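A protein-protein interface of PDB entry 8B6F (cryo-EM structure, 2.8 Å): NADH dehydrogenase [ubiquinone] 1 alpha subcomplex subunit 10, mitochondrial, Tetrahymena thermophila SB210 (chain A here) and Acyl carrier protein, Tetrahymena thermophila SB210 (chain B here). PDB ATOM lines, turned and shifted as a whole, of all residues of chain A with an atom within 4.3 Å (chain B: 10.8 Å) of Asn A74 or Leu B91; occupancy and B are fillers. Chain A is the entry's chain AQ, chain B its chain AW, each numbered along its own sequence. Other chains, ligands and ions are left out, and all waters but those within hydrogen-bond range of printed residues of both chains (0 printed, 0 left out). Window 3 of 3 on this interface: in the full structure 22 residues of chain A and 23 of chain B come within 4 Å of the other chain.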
ATOM      1  N   VAL A  36      26.945 -14.177   3.843  1.00  0.00           N
ATOM      2  CA  VAL A  36      27.723 -13.829   5.029  1.00  0.00           C
ATOM      3  C   VAL A  36      27.043 -14.354   6.287  1.00  0.00           C
ATOM      4  O   VAL A  36      27.683 -14.959   7.154  1.00  0.00           O
ATOM      5  CB  VAL A  36      27.942 -12.306   5.096  1.00  0.00           C
ATOM      6  CG1 VAL A  36      28.632 -11.916   6.396  1.00  0.00           C
ATOM      7  CG2 VAL A  36      28.752 -11.837   3.903  1.00  0.00           C
ATOM      8  N   TYR A  40      28.485 -17.193   8.790  1.00  0.00           N
ATOM      9  CA  TYR A  40      28.728 -16.854  10.187  1.00  0.00           C
ATOM     10  C   TYR A  40      27.998 -17.814  11.114  1.00  0.00           C
ATOM     11  O   TYR A  40      28.557 -18.268  12.118  1.00  0.00           O
ATOM     12  CB  TYR A  40      28.292 -15.413  10.455  1.00  0.00           C
ATOM     13  CG  TYR A  40      28.608 -14.909  11.846  1.00  0.00           C
ATOM     14  CD1 TYR A  40      29.836 -15.164  12.438  1.00  0.00           C
ATOM     15  CD2 TYR A  40      27.688 -14.151  12.552  1.00  0.00           C
ATOM     16  CE1 TYR A  40      30.130 -14.697  13.701  1.00  0.00           C
ATOM     17  CE2 TYR A  40      27.973 -13.677  13.817  1.00  0.00           C
ATOM     18  CZ  TYR A  40      29.196 -13.953  14.385  1.00  0.00           C
ATOM     19  OH  TYR A  40      29.482 -13.484  15.645  1.00  0.00           O
ATOM     20  N   GLY A  70      33.688 -13.175  15.107  1.00  0.00           N
ATOM     21  CA  GLY A  70      32.691 -12.127  14.965  1.00  0.00           C
ATOM     22  C   GLY A  70      33.256 -10.859  14.355  1.00  0.00           C
ATOM     23  O   GLY A  70      32.627 -10.243  13.491  1.00  0.00           O
ATOM     24  N   LYS A  71      34.445 -10.446  14.797  1.00  0.00           N
ATOM     25  CA  LYS A  71      35.082  -9.279  14.196  1.00  0.00           C
ATOM     26  C   LYS A  71      35.345  -9.509  12.713  1.00  0.00           C
ATOM     27  O   LYS A  71      35.078  -8.637  11.879  1.00  0.00           O
ATOM     28  CB  LYS A  71      36.384  -8.957  14.928  1.00  0.00           C
ATOM     29  CG  LYS A  71      36.188  -8.525  16.373  1.00  0.00           C
ATOM     30  CD  LYS A  71      37.505  -8.136  17.030  1.00  0.00           C
ATOM     31  CE  LYS A  71      38.450  -9.327  17.151  1.00  0.00           C
ATOM     32  NZ  LYS A  71      39.710  -8.970  17.866  1.00  0.00           N
ATOM     33  N   ASP A  72      35.871 -10.685  12.368  1.00  0.00           N
ATOM     34  CA  ASP A  72      36.165 -10.981  10.971  1.00  0.00           C
ATOM     35  C   ASP A  72      34.905 -10.957  10.120  1.00  0.00           C
ATOM     36  O   ASP A  72      34.913 -10.440   8.997  1.00  0.00           O
ATOM     37  CB  ASP A  72      36.851 -12.339  10.853  1.00  0.00           C
ATOM     38  CG  ASP A  72      38.308 -12.296  11.263  1.00  0.00           C
ATOM     39  OD1 ASP A  72      38.785 -11.213  11.660  1.00  0.00           O
ATOM     40  OD2 ASP A  72      38.977 -13.348  11.186  1.00  0.00           O
ATOM     41  N   PHE A  73      33.805 -11.505  10.639  1.00  0.00           N
ATOM     42  CA  PHE A  73      32.573 -11.545   9.861  1.00  0.00           C
ATOM     43  C   PHE A  73      31.929 -10.171   9.760  1.00  0.00           C
ATOM     44  O   PHE A  73      31.279  -9.870   8.754  1.00  0.00           O
ATOM     45  CB  PHE A  73      31.600 -12.560  10.457  1.00  0.00           C
ATOM     46  CG  PHE A  73      31.783 -13.951   9.921  1.00  0.00           C
ATOM     47  CD1 PHE A  73      31.203 -14.322   8.720  1.00  0.00           C
ATOM     48  CD2 PHE A  73      32.544 -14.881  10.605  1.00  0.00           C
ATOM     49  CE1 PHE A  73      31.372 -15.594   8.217  1.00  0.00           C
ATOM     50  CE2 PHE A  73      32.717 -16.156  10.107  1.00  0.00           C
ATOM     51  CZ  PHE A  73      32.129 -16.513   8.911  1.00  0.00           C
ATOM     52  N   ASN A  74      32.090  -9.325  10.779  1.00  0.00           N
ATOM     53  CA  ASN A  74      31.656  -7.941  10.634  1.00  0.00           C
ATOM     54  C   ASN A  74      32.412  -7.261   9.499  1.00  0.00           C
ATOM     55  O   ASN A  74      31.815  -6.550   8.683  1.00  0.00           O
ATOM     56  CB  ASN A  74      31.861  -7.176  11.942  1.00  0.00           C
ATOM     57  CG  ASN A  74      31.106  -7.789  13.102  1.00  0.00           C
ATOM     58  OD1 ASN A  74      30.187  -8.581  12.910  1.00  0.00           O
ATOM     59  ND2 ASN A  74      31.487  -7.417  14.318  1.00  0.00           N
ATOM     60  N   LYS A  75      33.730  -7.462   9.438  1.00  0.00           N
ATOM     61  CA  LYS A  75      34.511  -6.902   8.340  1.00  0.00           C
ATOM     62  C   LYS A  75      34.063  -7.476   7.002  1.00  0.00           C
ATOM     63  O   LYS A  75      33.959  -6.748   6.008  1.00  0.00           O
ATOM     64  CB  LYS A  75      36.001  -7.157   8.570  1.00  0.00           C
ATOM     65  CG  LYS A  75      36.658  -6.125   9.478  1.00  0.00           C
ATOM     66  CD  LYS A  75      38.121  -6.441   9.750  1.00  0.00           C
ATOM     67  CE  LYS A  75      38.266  -7.609  10.711  1.00  0.00           C
ATOM     68  NZ  LYS A  75      39.686  -7.845  11.098  1.00  0.00           N
ATOM     69  N   MET A  76      33.783  -8.781   6.959  1.00  0.00           N
ATOM     70  CA  MET A  76      33.322  -9.406   5.723  1.00  0.00           C
ATOM     71  C   MET A  76      32.018  -8.784   5.247  1.00  0.00           C
ATOM     72  O   MET A  76      31.856  -8.478   4.062  1.00  0.00           O
ATOM     73  CB  MET A  76      33.147 -10.912   5.925  1.00  0.00           C
ATOM     74  CG  MET A  76      34.442 -11.664   6.138  1.00  0.00           C
ATOM     75  SD  MET A  76      34.171 -13.313   6.809  1.00  0.00           S
ATOM     76  CE  MET A  76      33.220 -14.059   5.489  1.00  0.00           C
ATOM     77  N   LEU A  77      31.069  -8.592   6.165  1.00  0.00           N
ATOM     78  CA  LEU A  77      29.798  -7.984   5.790  1.00  0.00           C
ATOM     79  C   LEU A  77      29.997  -6.563   5.283  1.00  0.00           C
ATOM     80  O   LEU A  77      29.339  -6.138   4.327  1.00  0.00           O
ATOM     81  CB  LEU A  77      28.842  -8.005   6.982  1.00  0.00           C
ATOM     82  CG  LEU A  77      27.419  -7.510   6.718  1.00  0.00           C
ATOM     83  CD1 LEU A  77      26.744  -8.342   5.642  1.00  0.00           C
ATOM     84  CD2 LEU A  77      26.605  -7.546   7.997  1.00  0.00           C
ATOM     85  N   ALA A  78      30.901  -5.811   5.911  1.00  0.00           N
ATOM     86  CA  ALA A  78      31.201  -4.467   5.432  1.00  0.00           C
ATOM     87  C   ALA A  78      31.780  -4.497   4.023  1.00  0.00           C
ATOM     88  O   ALA A  78      31.480  -3.624   3.201  1.00  0.00           O
ATOM     89  CB  ALA A  78      32.166  -3.774   6.393  1.00  0.00           C
ATOM     90  N   HIS B  68      21.249  -9.786  25.152  1.00  0.00           N
ATOM     91  CA  HIS B  68      22.257  -9.345  24.200  1.00  0.00           C
ATOM     92  C   HIS B  68      22.729  -7.932  24.522  1.00  0.00           C
ATOM     93  O   HIS B  68      22.004  -7.127  25.111  1.00  0.00           O
ATOM     94  CB  HIS B  68      21.703  -9.399  22.776  1.00  0.00           C
ATOM     95  CG  HIS B  68      22.760  -9.520  21.722  1.00  0.00           C
ATOM     96  ND1 HIS B  68      23.497  -8.445  21.279  1.00  0.00           N
ATOM     97  CD2 HIS B  68      23.199 -10.591  21.021  1.00  0.00           C
ATOM     98  CE1 HIS B  68      24.348  -8.848  20.353  1.00  0.00           C
ATOM     99  NE2 HIS B  68      24.187 -10.147  20.177  1.00  0.00           N
ATOM    100  N   LYS B  70      23.734  -5.492  22.299  1.00  0.00           N
ATOM    101  CA  LYS B  70      23.193  -4.462  21.419  1.00  0.00           C
ATOM    102  C   LYS B  70      21.808  -4.015  21.862  1.00  0.00           C
ATOM    103  O   LYS B  70      21.458  -2.840  21.707  1.00  0.00           O
ATOM    104  CB  LYS B  70      23.148  -4.976  19.979  1.00  0.00           C
ATOM    105  CG  LYS B  70      24.515  -5.282  19.388  1.00  0.00           C
ATOM    106  CD  LYS B  70      25.351  -4.023  19.220  1.00  0.00           C
ATOM    107  CE  LYS B  70      26.680  -4.331  18.550  1.00  0.00           C
ATOM    108  NZ  LYS B  70      27.495  -3.102  18.340  1.00  0.00           N
ATOM    109  N   TRP B  83      13.203  -6.762  14.213  1.00  0.00           N
ATOM    110  CA  TRP B  83      14.553  -6.928  14.742  1.00  0.00           C
ATOM    111  C   TRP B  83      15.362  -5.644  14.605  1.00  0.00           C
ATOM    112  O   TRP B  83      16.078  -5.251  15.533  1.00  0.00           O
ATOM    113  CB  TRP B  83      15.249  -8.086  14.031  1.00  0.00           C
ATOM    114  CG  TRP B  83      14.467  -9.356  14.100  1.00  0.00           C
ATOM    115  CD1 TRP B  83      13.762  -9.938  13.091  1.00  0.00           C
ATOM    116  CD2 TRP B  83      14.302 -10.198  15.246  1.00  0.00           C
ATOM    117  NE1 TRP B  83      13.171 -11.095  13.537  1.00  0.00           N
ATOM    118  CE2 TRP B  83      13.488 -11.277  14.857  1.00  0.00           C
ATOM    119  CE3 TRP B  83      14.770 -10.145  16.563  1.00  0.00           C
ATOM    120  CZ2 TRP B  83      13.129 -12.295  15.736  1.00  0.00           C
ATOM    121  CZ3 TRP B  83      14.412 -11.156  17.436  1.00  0.00           C
ATOM    122  CH2 TRP B  83      13.598 -12.217  17.018  1.00  0.00           C
ATOM    123  N   SER B  84      15.266  -4.981  13.454  1.00  0.00           N
ATOM    124  CA  SER B  84      16.028  -3.755  13.238  1.00  0.00           C
ATOM    125  C   SER B  84      15.628  -2.666  14.226  1.00  0.00           C
ATOM    126  O   SER B  84      16.491  -1.967  14.771  1.00  0.00           O
ATOM    127  CB  SER B  84      15.840  -3.269  11.802  1.00  0.00           C
ATOM    128  OG  SER B  84      14.472  -3.025  11.520  1.00  0.00           O
ATOM    129  N   GLY B  87      16.786  -3.256  17.631  1.00  0.00           N
ATOM    130  CA  GLY B  87      18.222  -3.068  17.659  1.00  0.00           C
ATOM    131  C   GLY B  87      19.053  -4.285  17.312  1.00  0.00           C
ATOM    132  O   GLY B  87      20.276  -4.242  17.482  1.00  0.00           O
ATOM    133  N   VAL B  88      18.440  -5.363  16.830  1.00  0.00           N
ATOM    134  CA  VAL B  88      19.173  -6.576  16.487  1.00  0.00           C
ATOM    135  C   VAL B  88      19.713  -6.423  15.068  1.00  0.00           C
ATOM    136  O   VAL B  88      18.949  -6.358  14.103  1.00  0.00           O
ATOM    137  CB  VAL B  88      18.287  -7.822  16.615  1.00  0.00           C
ATOM    138  CG1 VAL B  88      19.017  -9.062  16.115  1.00  0.00           C
ATOM    139  CG2 VAL B  88      17.848  -8.012  18.056  1.00  0.00           C
ATOM    140  N   ASP B  89      21.037  -6.362  14.944  1.00  0.00           N
ATOM    141  CA  ASP B  89      21.677  -6.282  13.644  1.00  0.00           C
ATOM    142  C   ASP B  89      21.549  -7.617  12.915  1.00  0.00           C
ATOM    143  O   ASP B  89      21.264  -8.646  13.532  1.00  0.00           O
ATOM    144  CB  ASP B  89      23.148  -5.910  13.802  1.00  0.00           C
ATOM    145  CG  ASP B  89      23.339  -4.506  14.336  1.00  0.00           C
ATOM    146  OD1 ASP B  89      22.552  -3.613  13.959  1.00  0.00           O
ATOM    147  OD2 ASP B  89      24.272  -4.296  15.138  1.00  0.00           O
ATOM    148  N   PRO B  90      21.750  -7.629  11.595  1.00  0.00           N
ATOM    149  CA  PRO B  90      21.677  -8.912  10.876  1.00  0.00           C
ATOM    150  C   PRO B  90      22.641  -9.953  11.414  1.00  0.00           C
ATOM    151  O   PRO B  90      22.299 -11.141  11.449  1.00  0.00           O
ATOM    152  CB  PRO B  90      21.998  -8.521   9.423  1.00  0.00           C
ATOM    153  CG  PRO B  90      22.606  -7.158   9.499  1.00  0.00           C
ATOM    154  CD  PRO B  90      21.980  -6.500  10.679  1.00  0.00           C
ATOM    155  N   LEU B  91      23.842  -9.547  11.830  1.00  0.00           N
ATOM    156  CA  LEU B  91      24.793 -10.507  12.378  1.00  0.00           C
ATOM    157  C   LEU B  91      24.444 -10.888  13.811  1.00  0.00           C
ATOM    158  O   LEU B  91      24.616 -12.046  14.207  1.00  0.00           O
ATOM    159  CB  LEU B  91      26.216  -9.953  12.299  1.00  0.00           C
ATOM    160  CG  LEU B  91      26.814  -9.878  10.891  1.00  0.00           C
ATOM    161  CD1 LEU B  91      28.184  -9.240  10.929  1.00  0.00           C
ATOM    162  CD2 LEU B  91      26.900 -11.254  10.244  1.00  0.00           C
ATOM    163  N   SER B  92      23.960  -9.934  14.610  1.00  0.00           N
ATOM    164  CA  SER B  92      23.527 -10.273  15.960  1.00  0.00           C
ATOM    165  C   SER B  92      22.333 -11.214  15.931  1.00  0.00           C
ATOM    166  O   SER B  92      22.121 -11.981  16.877  1.00  0.00           O
ATOM    167  CB  SER B  92      23.178  -9.006  16.739  1.00  0.00           C
ATOM    168  OG  SER B  92      24.290  -8.132  16.813  1.00  0.00           O
ATOM    169  N   TYR B  93      21.543 -11.166  14.859  1.00  0.00           N
ATOM    170  CA  TYR B  93      20.363 -12.017  14.767  1.00  0.00           C
ATOM    171  C   TYR B  93      20.739 -13.494  14.759  1.00  0.00           C
ATOM    172  O   TYR B  93      20.079 -14.313  15.409  1.00  0.00           O
ATOM    173  CB  TYR B  93      19.564 -11.658  13.515  1.00  0.00           C
ATOM    174  CG  TYR B  93      18.361 -12.539  13.288  1.00  0.00           C
ATOM    175  CD1 TYR B  93      17.210 -12.388  14.050  1.00  0.00           C
ATOM    176  CD2 TYR B  93      18.372 -13.516  12.303  1.00  0.00           C
ATOM    177  CE1 TYR B  93      16.108 -13.192  13.843  1.00  0.00           C
ATOM    178  CE2 TYR B  93      17.275 -14.325  12.087  1.00  0.00           C
ATOM    179  CZ  TYR B  93      16.145 -14.158  12.860  1.00  0.00           C
ATOM    180  OH  TYR B  93      15.049 -14.959  12.649  1.00  0.00           O
ATOM    181  N   VAL B  94      21.803 -13.857  14.040  1.00  0.00           N
ATOM    182  CA  VAL B  94      22.176 -15.266  13.953  1.00  0.00           C
ATOM    183  C   VAL B  94      22.681 -15.767  15.299  1.00  0.00           C
ATOM    184  O   VAL B  94      22.426 -16.914  15.684  1.00  0.00           O
ATOM    185  CB  VAL B  94      23.209 -15.497  12.829  1.00  0.00           C
ATOM    186  CG1 VAL B  94      22.840 -14.715  11.569  1.00  0.00           C
ATOM    187  CG2 VAL B  94      24.623 -15.157  13.281  1.00  0.00           C
ATOM    188  N   GLU B  95      23.412 -14.927  16.034  1.00  0.00           N
ATOM    189  CA  GLU B  95      23.849 -15.312  17.372  1.00  0.00           C
ATOM    190  C   GLU B  95      22.655 -15.532  18.290  1.00  0.00           C
ATOM    191  O   GLU B  95      22.585 -16.532  19.011  1.00  0.00           O
ATOM    192  CB  GLU B  95      24.769 -14.239  17.953  1.00  0.00           C
ATOM    193  CG  GLU B  95      25.951 -13.888  17.074  1.00  0.00           C
ATOM    194  CD  GLU B  95      26.685 -12.660  17.567  1.00  0.00           C
ATOM    195  OE1 GLU B  95      26.280 -12.106  18.610  1.00  0.00           O
ATOM    196  OE2 GLU B  95      27.663 -12.245  16.912  1.00  0.00           O
ATOM    197  N   ILE B  96      21.704 -14.596  18.278  1.00  0.00           N
ATOM    198  CA  ILE B  96      20.529 -14.720  19.133  1.00  0.00           C
ATOM    199  C   ILE B  96      19.735 -15.964  18.762  1.00  0.00           C
ATOM    200  O   ILE B  96      19.186 -16.652  19.631  1.00  0.00           O
ATOM    201  CB  ILE B  96      19.671 -13.445  19.043  1.00  0.00           C
ATOM    202  CG1 ILE B  96      20.441 -12.256  19.622  1.00  0.00           C
ATOM    203  CG2 ILE B  96      18.347 -13.635  19.776  1.00  0.00           C
ATOM    204  CD1 ILE B  96      19.771 -10.915  19.402  1.00  0.00           C
ATOM    205  N   MET B  97      19.663 -16.275  17.468  1.00  0.00           N
ATOM    206  CA  MET B  97      18.895 -17.433  17.027  1.00  0.00           C
ATOM    207  C   MET B  97      19.597 -18.737  17.381  1.00  0.00           C
ATOM    208  O   MET B  97      18.937 -19.727  17.715  1.00  0.00           O
ATOM    209  CB  MET B  97      18.638 -17.349  15.526  1.00  0.00           C
ATOM    210  CG  MET B  97      17.638 -16.271  15.120  1.00  0.00           C
ATOM    211  SD  MET B  97      15.951 -16.533  15.718  1.00  0.00           S
ATOM    212  CE  MET B  97      15.964 -15.685  17.301  1.00  0.00           C
ATOM    213  N   LEU B  98      20.928 -18.767  17.320  1.00  0.00           N
ATOM    214  CA  LEU B  98      21.638 -19.959  17.772  1.00  0.00           C
ATOM    215  C   LEU B  98      21.396 -20.204  19.254  1.00  0.00           C
ATOM    216  O   LEU B  98      21.144 -21.341  19.669  1.00  0.00           O
ATOM    217  CB  LEU B  98      23.133 -19.827  17.488  1.00  0.00           C
ATOM    218  CG  LEU B  98      23.568 -19.952  16.027  1.00  0.00           C
ATOM    219  CD1 LEU B  98      25.043 -19.634  15.892  1.00  0.00           C
ATOM    220  CD2 LEU B  98      23.278 -21.344  15.493  1.00  0.00           C
ATOM    221  N   GLU B  99      21.473 -19.154  20.071  1.00  0.00           N
ATOM    222  CA  GLU B  99      21.205 -19.322  21.494  1.00  0.00           C
ATOM    223  C   GLU B  99      19.744 -19.668  21.745  1.00  0.00           C
ATOM    224  O   GLU B  99      19.434 -20.382  22.705  1.00  0.00           O
ATOM    225  CB  GLU B  99      21.600 -18.063  22.262  1.00  0.00           C
ATOM    226  CG  GLU B  99      23.098 -17.795  22.269  1.00  0.00           C
ATOM    227  CD  GLU B  99      23.913 -18.996  22.715  1.00  0.00           C
ATOM    228  OE1 GLU B  99      23.402 -19.799  23.522  1.00  0.00           O
ATOM    229  OE2 GLU B  99      25.063 -19.141  22.249  1.00  0.00           O
ATOM    230  N   LEU B 113      14.717 -19.028   9.478  1.00  0.00           N
ATOM    231  CA  LEU B 113      15.287 -17.882  10.180  1.00  0.00           C
ATOM    232  C   LEU B 113      15.268 -16.638   9.303  1.00  0.00           C
ATOM    233  O   LEU B 113      15.018 -15.529   9.789  1.00  0.00           O
ATOM    234  CB  LEU B 113      16.708 -18.206  10.638  1.00  0.00           C
ATOM    235  CG  LEU B 113      16.808 -19.352  11.648  1.00  0.00           C
ATOM    236  CD1 LEU B 113      18.248 -19.714  11.904  1.00  0.00           C
ATOM    237  CD2 LEU B 113      16.127 -18.982  12.951  1.00  0.00           C
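OH of Tyr A40 lies within hydrogen-bond range of OE2 of Glu B95 (2.5 Å).
O of Gly A70 lies close to OD1 of Asn A74, at 3.0 Å.
OE1 of Glu B95 is in hydrogen-bond range of NE2 of His B68 (3.3 Å).
Among the printed residues, merely in contact across the chains: Tyr A40 with Leu B91 (3.8 Å), Tyr A40 with Val B94 (3.3 Å), Phe A73 with Leu B91 (3.8 Å), Asn A74 with Leu B91 (2.9 Å) and Leu A77 with Leu B91 (3.7 Å).
Printed residues of chain B within 4 Å of Tyr A40: Leu B91, Val B94 and Glu B95.
No residue of chain B comes within 4 Å of Gly A70.
Printed residues of chain B within 4 Å of Phe A73: Leu B91.
Asn A74 touches one residue of chain B.
Lys A75 touches none of the printed residues of chain B.
Leu A77 touches just one residue of chain B: Leu B91.
Printed residues of chain A within 4 Å of Leu B91: Tyr A40, Phe A73, Asn A74 and Leu A77.
Ser B92 touches none of the printed residues of chain A.
Printed residues of chain A within 4 Å of Val B94: Tyr A40 (3.3 Å).
Of the printed residues of chain A, Glu B95 touches Tyr A40.
Along chain A the printed residues that touch a printed residue of chain B span positions 40 to 77.
Of the 18 printed residues of chain B, 3 touch a printed residue of chain A.
Among the printed residues, no Asp or Glu carboxylate lies within 4 Å of a Lys or Arg side-chain nitrogen of the other chain.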
